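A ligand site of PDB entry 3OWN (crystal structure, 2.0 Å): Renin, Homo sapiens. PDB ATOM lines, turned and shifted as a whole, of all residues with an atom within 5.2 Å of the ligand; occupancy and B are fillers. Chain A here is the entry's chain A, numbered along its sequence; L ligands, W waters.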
ATOM      1  N   THR A  18       6.860  13.889  24.183  1.00  0.00           N
ATOM      2  CA  THR A  18       5.442  13.904  24.045  1.00  0.00           C
ATOM      3  C   THR A  18       4.725  13.382  25.300  1.00  0.00           C
ATOM      4  O   THR A  18       3.556  13.718  25.528  1.00  0.00           O
ATOM      5  CB  THR A  18       4.977  13.065  22.838  1.00  0.00           C
ATOM      6  OG1 THR A  18       5.489  11.733  22.959  1.00  0.00           O
ATOM      7  CG2 THR A  18       5.464  13.651  21.544  1.00  0.00           C
ATOM      8  N   GLN A  19       5.413  12.557  26.106  1.00  0.00           N
ATOM      9  CA  GLN A  19       4.742  11.962  27.262  1.00  0.00           C
ATOM     10  C   GLN A  19       5.618  12.188  28.467  1.00  0.00           C
ATOM     11  O   GLN A  19       6.744  11.693  28.519  1.00  0.00           O
ATOM     12  CB  GLN A  19       4.483  10.462  27.050  1.00  0.00           C
ATOM     13  CG  GLN A  19       3.657  10.130  25.769  1.00  0.00           C
ATOM     14  CD  GLN A  19       3.460   8.640  25.597  1.00  0.00           C
ATOM     15  OE1 GLN A  19       3.415   8.126  24.465  1.00  0.00           O
ATOM     16  NE2 GLN A  19       3.367   7.923  26.705  1.00  0.00           N
ATOM     17  N   VAL A  36       0.204  10.384  34.074  1.00  0.00           N
ATOM     18  CA  VAL A  36       0.392  11.766  33.636  1.00  0.00           C
ATOM     19  C   VAL A  36      -0.334  12.650  34.645  1.00  0.00           C
ATOM     20  O   VAL A  36      -1.407  12.296  35.146  1.00  0.00           O
ATOM     21  CB  VAL A  36      -0.196  11.993  32.234  1.00  0.00           C
ATOM     22  CG1 VAL A  36      -0.290  13.502  31.826  1.00  0.00           C
ATOM     23  CG2 VAL A  36       0.679  11.299  31.272  1.00  0.00           C
ATOM     24  N   ASP A  38      -2.358  15.917  35.020  1.00  0.00           N
ATOM     25  CA  ASP A  38      -3.178  16.604  34.004  1.00  0.00           C
ATOM     26  C   ASP A  38      -3.976  17.772  34.604  1.00  0.00           C
ATOM     27  O   ASP A  38      -4.948  17.535  35.333  1.00  0.00           O
ATOM     28  CB  ASP A  38      -4.143  15.572  33.388  1.00  0.00           C
ATOM     29  CG  ASP A  38      -5.095  16.190  32.357  1.00  0.00           C
ATOM     30  OD1 ASP A  38      -4.767  17.238  31.774  1.00  0.00           O
ATOM     31  OD2 ASP A  38      -6.188  15.654  32.159  1.00  0.00           O
ATOM     32  N   GLY A  40      -5.783  19.644  32.903  1.00  0.00           N
ATOM     33  CA  GLY A  40      -7.010  19.732  32.138  1.00  0.00           C
ATOM     34  C   GLY A  40      -8.149  18.868  32.679  1.00  0.00           C
ATOM     35  O   GLY A  40      -9.260  18.930  32.187  1.00  0.00           O
ATOM     36  N   SER A  41      -7.888  18.082  33.723  1.00  0.00           N
ATOM     37  CA  SER A  41      -8.923  17.246  34.349  1.00  0.00           C
ATOM     38  C   SER A  41      -8.662  17.122  35.857  1.00  0.00           C
ATOM     39  O   SER A  41      -7.625  17.591  36.356  1.00  0.00           O
ATOM     40  CB  SER A  41      -9.006  15.850  33.668  1.00  0.00           C
ATOM     41  OG  SER A  41      -7.823  15.105  33.972  1.00  0.00           O
ATOM     42  N   ARG A  82     -14.851  11.259  30.028  1.00  0.00           N
ATOM     43  CA  ARG A  82     -14.754  11.614  28.625  1.00  0.00           C
ATOM     44  C   ARG A  82     -13.727  12.745  28.542  1.00  0.00           C
ATOM     45  O   ARG A  82     -13.918  13.813  29.108  1.00  0.00           O
ATOM     46  CB  ARG A  82     -16.128  12.007  28.048  1.00  0.00           C
ATOM     47  CG  ARG A  82     -17.151  10.840  27.971  1.00  0.00           C
ATOM     48  CD  ARG A  82     -18.588  11.307  27.724  1.00  0.00           C
ATOM     49  NE  ARG A  82     -19.544  10.209  28.026  1.00  0.00           N
ATOM     50  CZ  ARG A  82     -20.166   9.991  29.200  1.00  0.00           C
ATOM     51  NH1 ARG A  82     -19.975  10.780  30.260  1.00  0.00           N
ATOM     52  NH2 ARG A  82     -20.998   8.950  29.344  1.00  0.00           N
ATOM     53  N   TYR A  83     -12.612  12.471  27.896  1.00  0.00           N
ATOM     54  CA  TYR A  83     -11.633  13.518  27.601  1.00  0.00           C
ATOM     55  C   TYR A  83     -11.871  13.965  26.151  1.00  0.00           C
ATOM     56  O   TYR A  83     -12.626  13.332  25.422  1.00  0.00           O
ATOM     57  CB  TYR A  83     -10.201  12.985  27.741  1.00  0.00           C
ATOM     58  CG  TYR A  83      -9.858  12.540  29.155  1.00  0.00           C
ATOM     59  CD1 TYR A  83      -9.561  13.469  30.158  1.00  0.00           C
ATOM     60  CD2 TYR A  83      -9.830  11.192  29.480  1.00  0.00           C
ATOM     61  CE1 TYR A  83      -9.236  13.060  31.445  1.00  0.00           C
ATOM     62  CE2 TYR A  83      -9.529  10.771  30.754  1.00  0.00           C
ATOM     63  CZ  TYR A  83      -9.206  11.700  31.731  1.00  0.00           C
ATOM     64  OH  TYR A  83      -8.870  11.242  32.972  1.00  0.00           O
ATOM     65  N   SER A  84     -11.240  15.064  25.730  1.00  0.00           N
ATOM     66  CA  SER A  84     -11.402  15.517  24.352  1.00  0.00           C
ATOM     67  C   SER A  84     -10.913  14.474  23.310  1.00  0.00           C
ATOM     68  O   SER A  84     -11.428  14.361  22.190  1.00  0.00           O
ATOM     69  CB  SER A  84     -10.708  16.876  24.182  1.00  0.00           C
ATOM     70  OG  SER A  84     -10.830  17.336  22.830  1.00  0.00           O
ATOM     71  N   THR A  85      -9.905  13.701  23.692  1.00  0.00           N
ATOM     72  CA  THR A  85      -9.310  12.781  22.738  1.00  0.00           C
ATOM     73  C   THR A  85      -9.445  11.303  23.100  1.00  0.00           C
ATOM     74  O   THR A  85      -8.842  10.421  22.488  1.00  0.00           O
ATOM     75  CB  THR A  85      -7.843  13.178  22.545  1.00  0.00           C
ATOM     76  OG1 THR A  85      -7.227  13.183  23.842  1.00  0.00           O
ATOM     77  CG2 THR A  85      -7.749  14.633  21.936  1.00  0.00           C
ATOM     78  N   PRO A 118      -6.442   6.163  22.684  1.00  0.00           N
ATOM     79  CA  PRO A 118      -5.018   6.213  22.493  1.00  0.00           C
ATOM     80  C   PRO A 118      -4.166   5.341  23.438  1.00  0.00           C
ATOM     81  O   PRO A 118      -2.956   5.432  23.384  1.00  0.00           O
ATOM     82  CB  PRO A 118      -4.701   7.671  22.777  1.00  0.00           C
ATOM     83  CG  PRO A 118      -5.620   7.980  23.916  1.00  0.00           C
ATOM     84  CD  PRO A 118      -6.896   7.222  23.618  1.00  0.00           C
ATOM     85  N   PHE A 119      -4.765   4.497  24.269  1.00  0.00           N
ATOM     86  CA  PHE A 119      -3.973   3.930  25.394  1.00  0.00           C
ATOM     87  C   PHE A 119      -2.916   2.907  25.093  1.00  0.00           C
ATOM     88  O   PHE A 119      -1.947   2.809  25.831  1.00  0.00           O
ATOM     89  CB  PHE A 119      -4.881   3.520  26.561  1.00  0.00           C
ATOM     90  CG  PHE A 119      -5.768   4.643  27.021  1.00  0.00           C
ATOM     91  CD1 PHE A 119      -5.252   5.625  27.869  1.00  0.00           C
ATOM     92  CD2 PHE A 119      -7.081   4.739  26.578  1.00  0.00           C
ATOM     93  CE1 PHE A 119      -6.049   6.650  28.289  1.00  0.00           C
ATOM     94  CE2 PHE A 119      -7.864   5.801  26.996  1.00  0.00           C
ATOM     95  CZ  PHE A 119      -7.348   6.750  27.837  1.00  0.00           C
ATOM     96  N   LEU A 121      -0.839   3.357  22.958  1.00  0.00           N
ATOM     97  CA  LEU A 121       0.237   4.246  22.517  1.00  0.00           C
ATOM     98  C   LEU A 121       0.889   5.003  23.657  1.00  0.00           C
ATOM     99  O   LEU A 121       1.902   5.698  23.476  1.00  0.00           O
ATOM    100  CB  LEU A 121      -0.344   5.283  21.548  1.00  0.00           C
ATOM    101  CG  LEU A 121      -0.425   5.072  20.032  1.00  0.00           C
ATOM    102  CD1 LEU A 121      -0.415   3.646  19.560  1.00  0.00           C
ATOM    103  CD2 LEU A 121      -1.511   5.898  19.341  1.00  0.00           C
ATOM    104  N   ALA A 122       0.273   4.890  24.833  1.00  0.00           N
ATOM    105  CA  ALA A 122       0.720   5.586  26.029  1.00  0.00           C
ATOM    106  C   ALA A 122       1.746   4.740  26.774  1.00  0.00           C
ATOM    107  O   ALA A 122       1.547   3.527  26.953  1.00  0.00           O
ATOM    108  CB  ALA A 122      -0.498   5.840  26.915  1.00  0.00           C
ATOM    109  N   PHE A 124       2.471   5.487  29.872  1.00  0.00           N
ATOM    110  CA  PHE A 124       1.974   5.527  31.245  1.00  0.00           C
ATOM    111  C   PHE A 124       0.690   4.718  31.376  1.00  0.00           C
ATOM    112  O   PHE A 124       0.020   4.367  30.394  1.00  0.00           O
ATOM    113  CB  PHE A 124       1.751   6.969  31.736  1.00  0.00           C
ATOM    114  CG  PHE A 124       0.949   7.789  30.772  1.00  0.00           C
ATOM    115  CD1 PHE A 124       1.590   8.484  29.756  1.00  0.00           C
ATOM    116  CD2 PHE A 124      -0.439   7.852  30.868  1.00  0.00           C
ATOM    117  CE1 PHE A 124       0.856   9.248  28.837  1.00  0.00           C
ATOM    118  CE2 PHE A 124      -1.186   8.621  29.977  1.00  0.00           C
ATOM    119  CZ  PHE A 124      -0.536   9.302  28.943  1.00  0.00           C
ATOM    120  N   VAL A 127      -3.964   8.432  34.990  1.00  0.00           N
ATOM    121  CA  VAL A 127      -3.993   9.885  35.011  1.00  0.00           C
ATOM    122  C   VAL A 127      -4.265  10.408  36.430  1.00  0.00           C
ATOM    123  O   VAL A 127      -5.097   9.861  37.123  1.00  0.00           O
ATOM    124  CB  VAL A 127      -5.074  10.457  34.006  1.00  0.00           C
ATOM    125  CG1 VAL A 127      -5.235  12.027  34.171  1.00  0.00           C
ATOM    126  CG2 VAL A 127      -4.704  10.035  32.553  1.00  0.00           C
ATOM    127  N   GLN A 135     -14.504  20.555  37.829  1.00  0.00           N
ATOM    128  CA  GLN A 135     -14.361  19.714  36.661  1.00  0.00           C
ATOM    129  C   GLN A 135     -14.275  18.215  36.955  1.00  0.00           C
ATOM    130  O   GLN A 135     -14.197  17.425  36.016  1.00  0.00           O
ATOM    131  CB  GLN A 135     -13.151  20.137  35.830  1.00  0.00           C
ATOM    132  CG  GLN A 135     -13.228  21.550  35.250  1.00  0.00           C
ATOM    133  CD  GLN A 135     -14.459  21.722  34.376  1.00  0.00           C
ATOM    134  OE1 GLN A 135     -15.275  22.631  34.600  1.00  0.00           O
ATOM    135  NE2 GLN A 135     -14.635  20.824  33.429  1.00  0.00           N
ATOM    136  N   ILE A 137     -15.463  14.523  37.666  1.00  0.00           N
ATOM    137  CA  ILE A 137     -16.629  13.732  37.285  1.00  0.00           C
ATOM    138  C   ILE A 137     -16.994  12.961  38.540  1.00  0.00           C
ATOM    139  O   ILE A 137     -16.112  12.478  39.266  1.00  0.00           O
ATOM    140  CB  ILE A 137     -16.324  12.766  36.099  1.00  0.00           C
ATOM    141  CG1 ILE A 137     -15.876  13.560  34.854  1.00  0.00           C
ATOM    142  CG2 ILE A 137     -17.505  11.843  35.777  1.00  0.00           C
ATOM    143  CD1 ILE A 137     -16.841  14.711  34.408  1.00  0.00           C
ATOM    144  N   LEU A 224      -6.432  27.396  27.888  1.00  0.00           N
ATOM    145  CA  LEU A 224      -6.464  26.421  28.965  1.00  0.00           C
ATOM    146  C   LEU A 224      -5.020  25.851  29.080  1.00  0.00           C
ATOM    147  O   LEU A 224      -4.462  25.319  28.109  1.00  0.00           O
ATOM    148  CB  LEU A 224      -7.462  25.321  28.582  1.00  0.00           C
ATOM    149  CG  LEU A 224      -7.910  24.178  29.521  1.00  0.00           C
ATOM    150  CD1 LEU A 224      -6.867  23.502  30.468  1.00  0.00           C
ATOM    151  CD2 LEU A 224      -9.230  24.529  30.212  1.00  0.00           C
ATOM    152  N   ASP A 226      -2.762  23.159  29.940  1.00  0.00           N
ATOM    153  CA  ASP A 226      -3.044  21.717  29.984  1.00  0.00           C
ATOM    154  C   ASP A 226      -1.768  20.867  30.036  1.00  0.00           C
ATOM    155  O   ASP A 226      -1.176  20.523  29.015  1.00  0.00           O
ATOM    156  CB  ASP A 226      -3.858  21.349  28.739  1.00  0.00           C
ATOM    157  CG  ASP A 226      -4.511  19.983  28.844  1.00  0.00           C
ATOM    158  OD1 ASP A 226      -4.389  19.312  29.869  1.00  0.00           O
ATOM    159  OD2 ASP A 226      -5.151  19.600  27.869  1.00  0.00           O
ATOM    160  N   GLY A 228      -1.637  17.769  30.699  1.00  0.00           N
ATOM    161  CA  GLY A 228      -1.949  16.430  30.152  1.00  0.00           C
ATOM    162  C   GLY A 228      -2.184  16.363  28.643  1.00  0.00           C
ATOM    163  O   GLY A 228      -2.863  15.461  28.150  1.00  0.00           O
ATOM    164  N   ALA A 229      -1.607  17.313  27.911  1.00  0.00           N
ATOM    165  CA  ALA A 229      -1.672  17.460  26.440  1.00  0.00           C
ATOM    166  C   ALA A 229      -0.217  17.706  25.995  1.00  0.00           C
ATOM    167  O   ALA A 229       0.522  18.512  26.565  1.00  0.00           O
ATOM    168  CB  ALA A 229      -2.557  18.700  26.029  1.00  0.00           C
ATOM    169  N   SER A 230       0.215  17.005  24.958  1.00  0.00           N
ATOM    170  CA  SER A 230       1.599  17.202  24.506  1.00  0.00           C
ATOM    171  C   SER A 230       1.849  18.477  23.741  1.00  0.00           C
ATOM    172  O   SER A 230       2.991  18.880  23.622  1.00  0.00           O
ATOM    173  CB  SER A 230       2.075  16.072  23.602  1.00  0.00           C
ATOM    174  OG  SER A 230       1.875  14.817  24.251  1.00  0.00           O
ATOM    175  N   TYR A 231       0.800  19.036  23.137  1.00  0.00           N
ATOM    176  CA  TYR A 231       0.968  20.058  22.117  1.00  0.00           C
ATOM    177  C   TYR A 231       0.160  21.298  22.437  1.00  0.00           C
ATOM    178  O   TYR A 231      -0.411  21.400  23.501  1.00  0.00           O
ATOM    179  CB  TYR A 231       0.588  19.556  20.702  1.00  0.00           C
ATOM    180  CG  TYR A 231       1.086  18.166  20.420  1.00  0.00           C
ATOM    181  CD1 TYR A 231       2.453  17.918  20.296  1.00  0.00           C
ATOM    182  CD2 TYR A 231       0.195  17.097  20.285  1.00  0.00           C
ATOM    183  CE1 TYR A 231       2.928  16.666  20.060  1.00  0.00           C
ATOM    184  CE2 TYR A 231       0.654  15.809  20.070  1.00  0.00           C
ATOM    185  CZ  TYR A 231       2.025  15.602  19.952  1.00  0.00           C
ATOM    186  OH  TYR A 231       2.525  14.342  19.741  1.00  0.00           O
ATOM    187  N   ILE A 232       0.172  22.220  21.482  1.00  0.00           N
ATOM    188  CA  ILE A 232      -0.638  23.422  21.551  1.00  0.00           C
ATOM    189  C   ILE A 232      -1.805  23.214  20.556  1.00  0.00           C
ATOM    190  O   ILE A 232      -1.614  22.687  19.470  1.00  0.00           O
ATOM    191  CB  ILE A 232       0.192  24.672  21.177  1.00  0.00           C
ATOM    192  CG1 ILE A 232       1.240  24.949  22.312  1.00  0.00           C
ATOM    193  CG2 ILE A 232      -0.756  25.863  20.903  1.00  0.00           C
ATOM    194  CD1 ILE A 232       2.187  26.060  21.966  1.00  0.00           C
ATOM    195  N   SER A 233      -3.005  23.577  20.960  1.00  0.00           N
ATOM    196  CA  SER A 233      -4.125  23.450  20.056  1.00  0.00           C
ATOM    197  C   SER A 233      -4.961  24.724  20.054  1.00  0.00           C
ATOM    198  O   SER A 233      -4.971  25.478  21.016  1.00  0.00           O
ATOM    199  CB  SER A 233      -5.005  22.251  20.449  1.00  0.00           C
ATOM    200  OG  SER A 233      -5.653  22.514  21.671  1.00  0.00           O
ATOM    201  N   HIS A 301      -2.108  21.379  17.009  1.00  0.00           N
ATOM    202  CA  HIS A 301      -3.303  20.641  16.599  1.00  0.00           C
ATOM    203  C   HIS A 301      -4.587  21.455  16.701  1.00  0.00           C
ATOM    204  O   HIS A 301      -4.608  22.524  17.292  1.00  0.00           O
ATOM    205  CB  HIS A 301      -3.420  19.326  17.387  1.00  0.00           C
ATOM    206  CG  HIS A 301      -2.363  18.334  17.033  1.00  0.00           C
ATOM    207  ND1 HIS A 301      -1.092  18.396  17.559  1.00  0.00           N
ATOM    208  CD2 HIS A 301      -2.351  17.304  16.154  1.00  0.00           C
ATOM    209  CE1 HIS A 301      -0.337  17.437  17.026  1.00  0.00           C
ATOM    210  NE2 HIS A 301      -1.088  16.757  16.180  1.00  0.00           N
ATOM    211  N   ALA A 302      -5.642  20.916  16.103  1.00  0.00           N
ATOM    212  CA  ALA A 302      -7.007  21.397  16.210  1.00  0.00           C
ATOM    213  C   ALA A 302      -7.669  20.649  17.359  1.00  0.00           C
ATOM    214  O   ALA A 302      -7.607  19.421  17.436  1.00  0.00           O
ATOM    215  CB  ALA A 302      -7.815  21.133  14.906  1.00  0.00           C
ATOM    216  N   MET A 303      -8.248  21.391  18.279  1.00  0.00           N
ATOM    217  CA  MET A 303      -9.046  20.765  19.287  1.00  0.00           C
ATOM    218  C   MET A 303     -10.235  21.645  19.601  1.00  0.00           C
ATOM    219  O   MET A 303     -10.093  22.758  20.090  1.00  0.00           O
ATOM    220  CB  MET A 303      -8.223  20.436  20.550  1.00  0.00           C
ATOM    221  CG  MET A 303      -9.055  19.760  21.648  1.00  0.00           C
ATOM    222  SD  MET A 303      -8.108  19.230  23.137  1.00  0.00           S
ATOM    223  CE  MET A 303      -7.648  20.766  23.933  1.00  0.00           C
ATOM    224  N   ILE A 305     -13.297  22.243  21.984  1.00  0.00           N
ATOM    225  CA  ILE A 305     -13.867  21.966  23.292  1.00  0.00           C
ATOM    226  C   ILE A 305     -15.197  22.688  23.282  1.00  0.00           C
ATOM    227  O   ILE A 305     -15.233  23.902  23.028  1.00  0.00           O
ATOM    228  CB  ILE A 305     -12.980  22.509  24.493  1.00  0.00           C
ATOM    229  CG1 ILE A 305     -11.675  21.714  24.616  1.00  0.00           C
ATOM    230  CG2 ILE A 305     -13.703  22.397  25.846  1.00  0.00           C
ATOM    231  CD1 ILE A 305     -10.587  22.290  23.816  1.00  0.00           C
ATOM    232  N   THR A 309     -16.614  25.352  28.640  1.00  0.00           N
ATOM    233  CA  THR A 309     -15.148  25.479  28.743  1.00  0.00           C
ATOM    234  C   THR A 309     -14.544  26.075  27.486  1.00  0.00           C
ATOM    235  O   THR A 309     -13.689  26.964  27.570  1.00  0.00           O
ATOM    236  CB  THR A 309     -14.466  24.155  29.152  1.00  0.00           C
ATOM    237  OG1 THR A 309     -15.033  23.704  30.382  1.00  0.00           O
ATOM    238  CG2 THR A 309     -12.939  24.379  29.357  1.00  0.00           C
ATOM    239  N   ALA A 314      -5.493  25.350  23.840  1.00  0.00           N
ATOM    240  CA  ALA A 314      -4.928  24.623  24.994  1.00  0.00           C
ATOM    241  C   ALA A 314      -3.404  24.723  24.895  1.00  0.00           C
ATOM    242  O   ALA A 314      -2.836  24.548  23.816  1.00  0.00           O
ATOM    243  CB  ALA A 314      -5.356  23.150  25.009  1.00  0.00           C
HETATM  244  N1  LIG L   1      -5.908  15.626  27.194  1.00  0.00           N
HETATM  245  C1  LIG L   1      -6.773  15.317  28.329  1.00  0.00           C
HETATM  246  C2  LIG L   1      -7.298  16.557  29.066  1.00  0.00           C
HETATM  247  C3  LIG L   1      -8.204  17.363  28.108  1.00  0.00           C
HETATM  248  C4  LIG L   1      -9.253  18.243  28.797  1.00  0.00           C
HETATM  249  C5  LIG L   1     -10.408  17.328  29.137  1.00  0.00           C
HETATM  250  C6  LIG L   1      -5.939  14.387  29.246  1.00  0.00           C
HETATM  251  O1  LIG L   1      -6.233  17.388  29.550  1.00  0.00           O
HETATM  252  C7  LIG L   1      -9.689  19.409  27.889  1.00  0.00           C
HETATM  253  C8  LIG L   1      -8.548  20.394  27.592  1.00  0.00           C
HETATM  254  C9  LIG L   1     -10.888  20.161  28.485  1.00  0.00           C
HETATM  255  O2  LIG L   1     -10.950  16.717  28.235  1.00  0.00           O
HETATM  256  O3  LIG L   1      -5.428  13.249  28.560  1.00  0.00           O
HETATM  257  C10 LIG L   1     -11.860  16.346  30.909  1.00  0.00           C
HETATM  258  C11 LIG L   1     -13.013  17.186  31.424  1.00  0.00           C
HETATM  259  C12 LIG L   1     -14.070  16.206  31.935  1.00  0.00           C
HETATM  260  C13 LIG L   1     -12.600  18.181  32.519  1.00  0.00           C
HETATM  261  N2  LIG L   1     -10.775  17.198  30.402  1.00  0.00           N
HETATM  262  C14 LIG L   1      -5.260  15.763  24.906  1.00  0.00           C
HETATM  263  C15 LIG L   1      -5.286  16.643  23.828  1.00  0.00           C
HETATM  264  C16 LIG L   1      -4.192  16.670  22.952  1.00  0.00           C
HETATM  265  C17 LIG L   1      -3.100  15.817  23.119  1.00  0.00           C
HETATM  266  C18 LIG L   1      -3.095  14.891  24.157  1.00  0.00           C
HETATM  267  C19 LIG L   1      -4.185  14.873  25.033  1.00  0.00           C
HETATM  268  C20 LIG L   1      -6.328  15.580  25.920  1.00  0.00           C
HETATM  269  C21 LIG L   1      -1.954  13.958  24.429  1.00  0.00           C
HETATM  270  N3  LIG L   1      -4.194  17.627  21.901  1.00  0.00           N
HETATM  271  C22 LIG L   1      -5.259  17.488  20.905  1.00  0.00           C
HETATM  272  S1  LIG L   1      -3.245  18.843  21.953  1.00  0.00           S
HETATM  273  C23 LIG L   1      -1.867  18.442  22.673  1.00  0.00           C
HETATM  274  O4  LIG L   1      -0.799  14.325  24.346  1.00  0.00           O
HETATM  275  O5  LIG L   1      -7.488  15.322  25.588  1.00  0.00           O
HETATM  276  O6  LIG L   1      -3.873  19.879  22.782  1.00  0.00           O
HETATM  277  O7  LIG L   1      -3.010  19.384  20.646  1.00  0.00           O
HETATM  278  N4  LIG L   1      -2.299  12.739  24.750  1.00  0.00           N
HETATM  279  C24 LIG L   1      -1.601  11.562  25.251  1.00  0.00           C
HETATM  280  C25 LIG L   1      -2.452  11.000  26.327  1.00  0.00           C
HETATM  281  C26 LIG L   1      -3.823  11.540  28.253  1.00  0.00           C
HETATM  282  C27 LIG L   1      -4.204  10.189  28.315  1.00  0.00           C
HETATM  283  C28 LIG L   1      -3.733   9.263  27.374  1.00  0.00           C
HETATM  284  C29 LIG L   1      -2.870   9.683  26.361  1.00  0.00           C
HETATM  285  C30 LIG L   1      -2.962  11.950  27.231  1.00  0.00           C
HETATM  286  C31 LIG L   1      -4.399  12.507  29.257  1.00  0.00           C
HETATM  287  C32 LIG L   1      -1.242  10.567  24.187  1.00  0.00           C
HETATM  288  C33 LIG L   1      -2.053  10.351  23.061  1.00  0.00           C
HETATM  289  C34 LIG L   1      -1.695   9.444  22.071  1.00  0.00           C
HETATM  290  C35 LIG L   1      -0.492   8.730  22.203  1.00  0.00           C
HETATM  291  C36 LIG L   1       0.323   8.945  23.309  1.00  0.00           C
HETATM  292  C37 LIG L   1      -0.044   9.855  24.297  1.00  0.00           C
HETATM  293  O   HOH W   1      -7.827  16.960  19.041  1.00  0.00           O
HETATM  294  O   HOH W   2     -13.449  17.535  27.388  1.00  0.00           O
HETATM  295  O   HOH W   3      -5.136  11.957  24.063  1.00  0.00           O
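Gln 19 touches the ligand (OE1 to C36, 3.4 Å). Ser 41 touches the ligand (CB to N2, 3.95 Å). Arg 82 touches the ligand (O to C12, 3.7 Å). CA of Tyr 83 touches O2 of the ligand, 3.3 Å away. Pro 118 touches the ligand (CB to C34, 3.6 Å). Phe 119 touches the ligand. Leu 121 touches the ligand. CZ of Phe 124 touches C29 of the ligand (3.5 Å). Gln 135 touches the ligand (NE2 to C13, 3.5 Å). CB of Ala 229 touches C23 of the ligand (3.4 Å). Tyr 231 touches the ligand (N to C23, 2.8 Å). Ile 232 touches the ligand. His 301 touches the ligand (CB to O7, 3.3 Å). Met 303 touches the ligand. Hydrophobic or aromatic side chains within 4 Å of the ligand: Tyr 83, Pro 118, Phe 119, Leu 121, Phe 124, Ala 229, Tyr 231, His 301 and Met 303. The nearest printed residue that does not touch the ligand is Ile 137 (4.004 Å).
Water W3 lies within hydrogen-bond range of OG1 of Thr 85 (2.4 Å) and N4 of the ligand (3.0 Å).
The backbone NH (N) of Thr 85 is in hydrogen-bond range of an oxygen (O5) of the ligand. N of Ser 230 sits at hydrogen-bond distance from O4 of the ligand (2.9 Å). The side-chain hydroxyl (OG) of Ser 233 lies within hydrogen-bond range of an oxygen (O6) of the ligand. A nitrogen (N2) of the ligand is in hydrogen-bond range of the backbone carbonyl oxygen of Gly 40. N1 of the ligand sits at hydrogen-bond distance from O of Gly 228 (3.2 Å). OD1 of Asp 226 sits at hydrogen-bond distance from O1 of the ligand, at 2.7 Å. The side-chain hydroxyl of Ser 230 is in hydrogen-bond range of an oxygen (O4) of the ligand (2.7 Å). OG1 of Thr 85 is in hydrogen-bond range of O5 of the ligand. The backbone NH (N) of Ser 84 sits at hydrogen-bond distance from an oxygen (O2) of the ligand (3.0 Å). OD1 of Asp 38 sits at hydrogen-bond distance from O1 of the ligand (2.7 Å).
The side-chain carboxylate of Asp 226 lies within hydrogen-bond range of the backbone NH of Gly 40 (3.4 Å). N of Gly 228 lies close to OD1 of Asp 38 (3.4 Å). OE1 of Gln 19 lies close to O of Leu 121 (3.0 Å). OG of Ser 41 lies within hydrogen-bond range of OD2 of Asp 38. The backbone NH of His 301 lies within hydrogen-bond range of the backbone carbonyl oxygen of Ile 232, 2.8 Å away. The side-chain sulfur of Met 303 lies close to the side-chain hydroxyl of Ser 84 (3.3 Å). The side-chain carboxylate (OD1) of Asp 226 sits close to the backbone NH (N) of Gly 228 (3.3 Å). The backbone carbonyl oxygen (O) of Ser 233 is in hydrogen-bond range of the backbone NH (N) of Ala 314 (2.9 Å).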
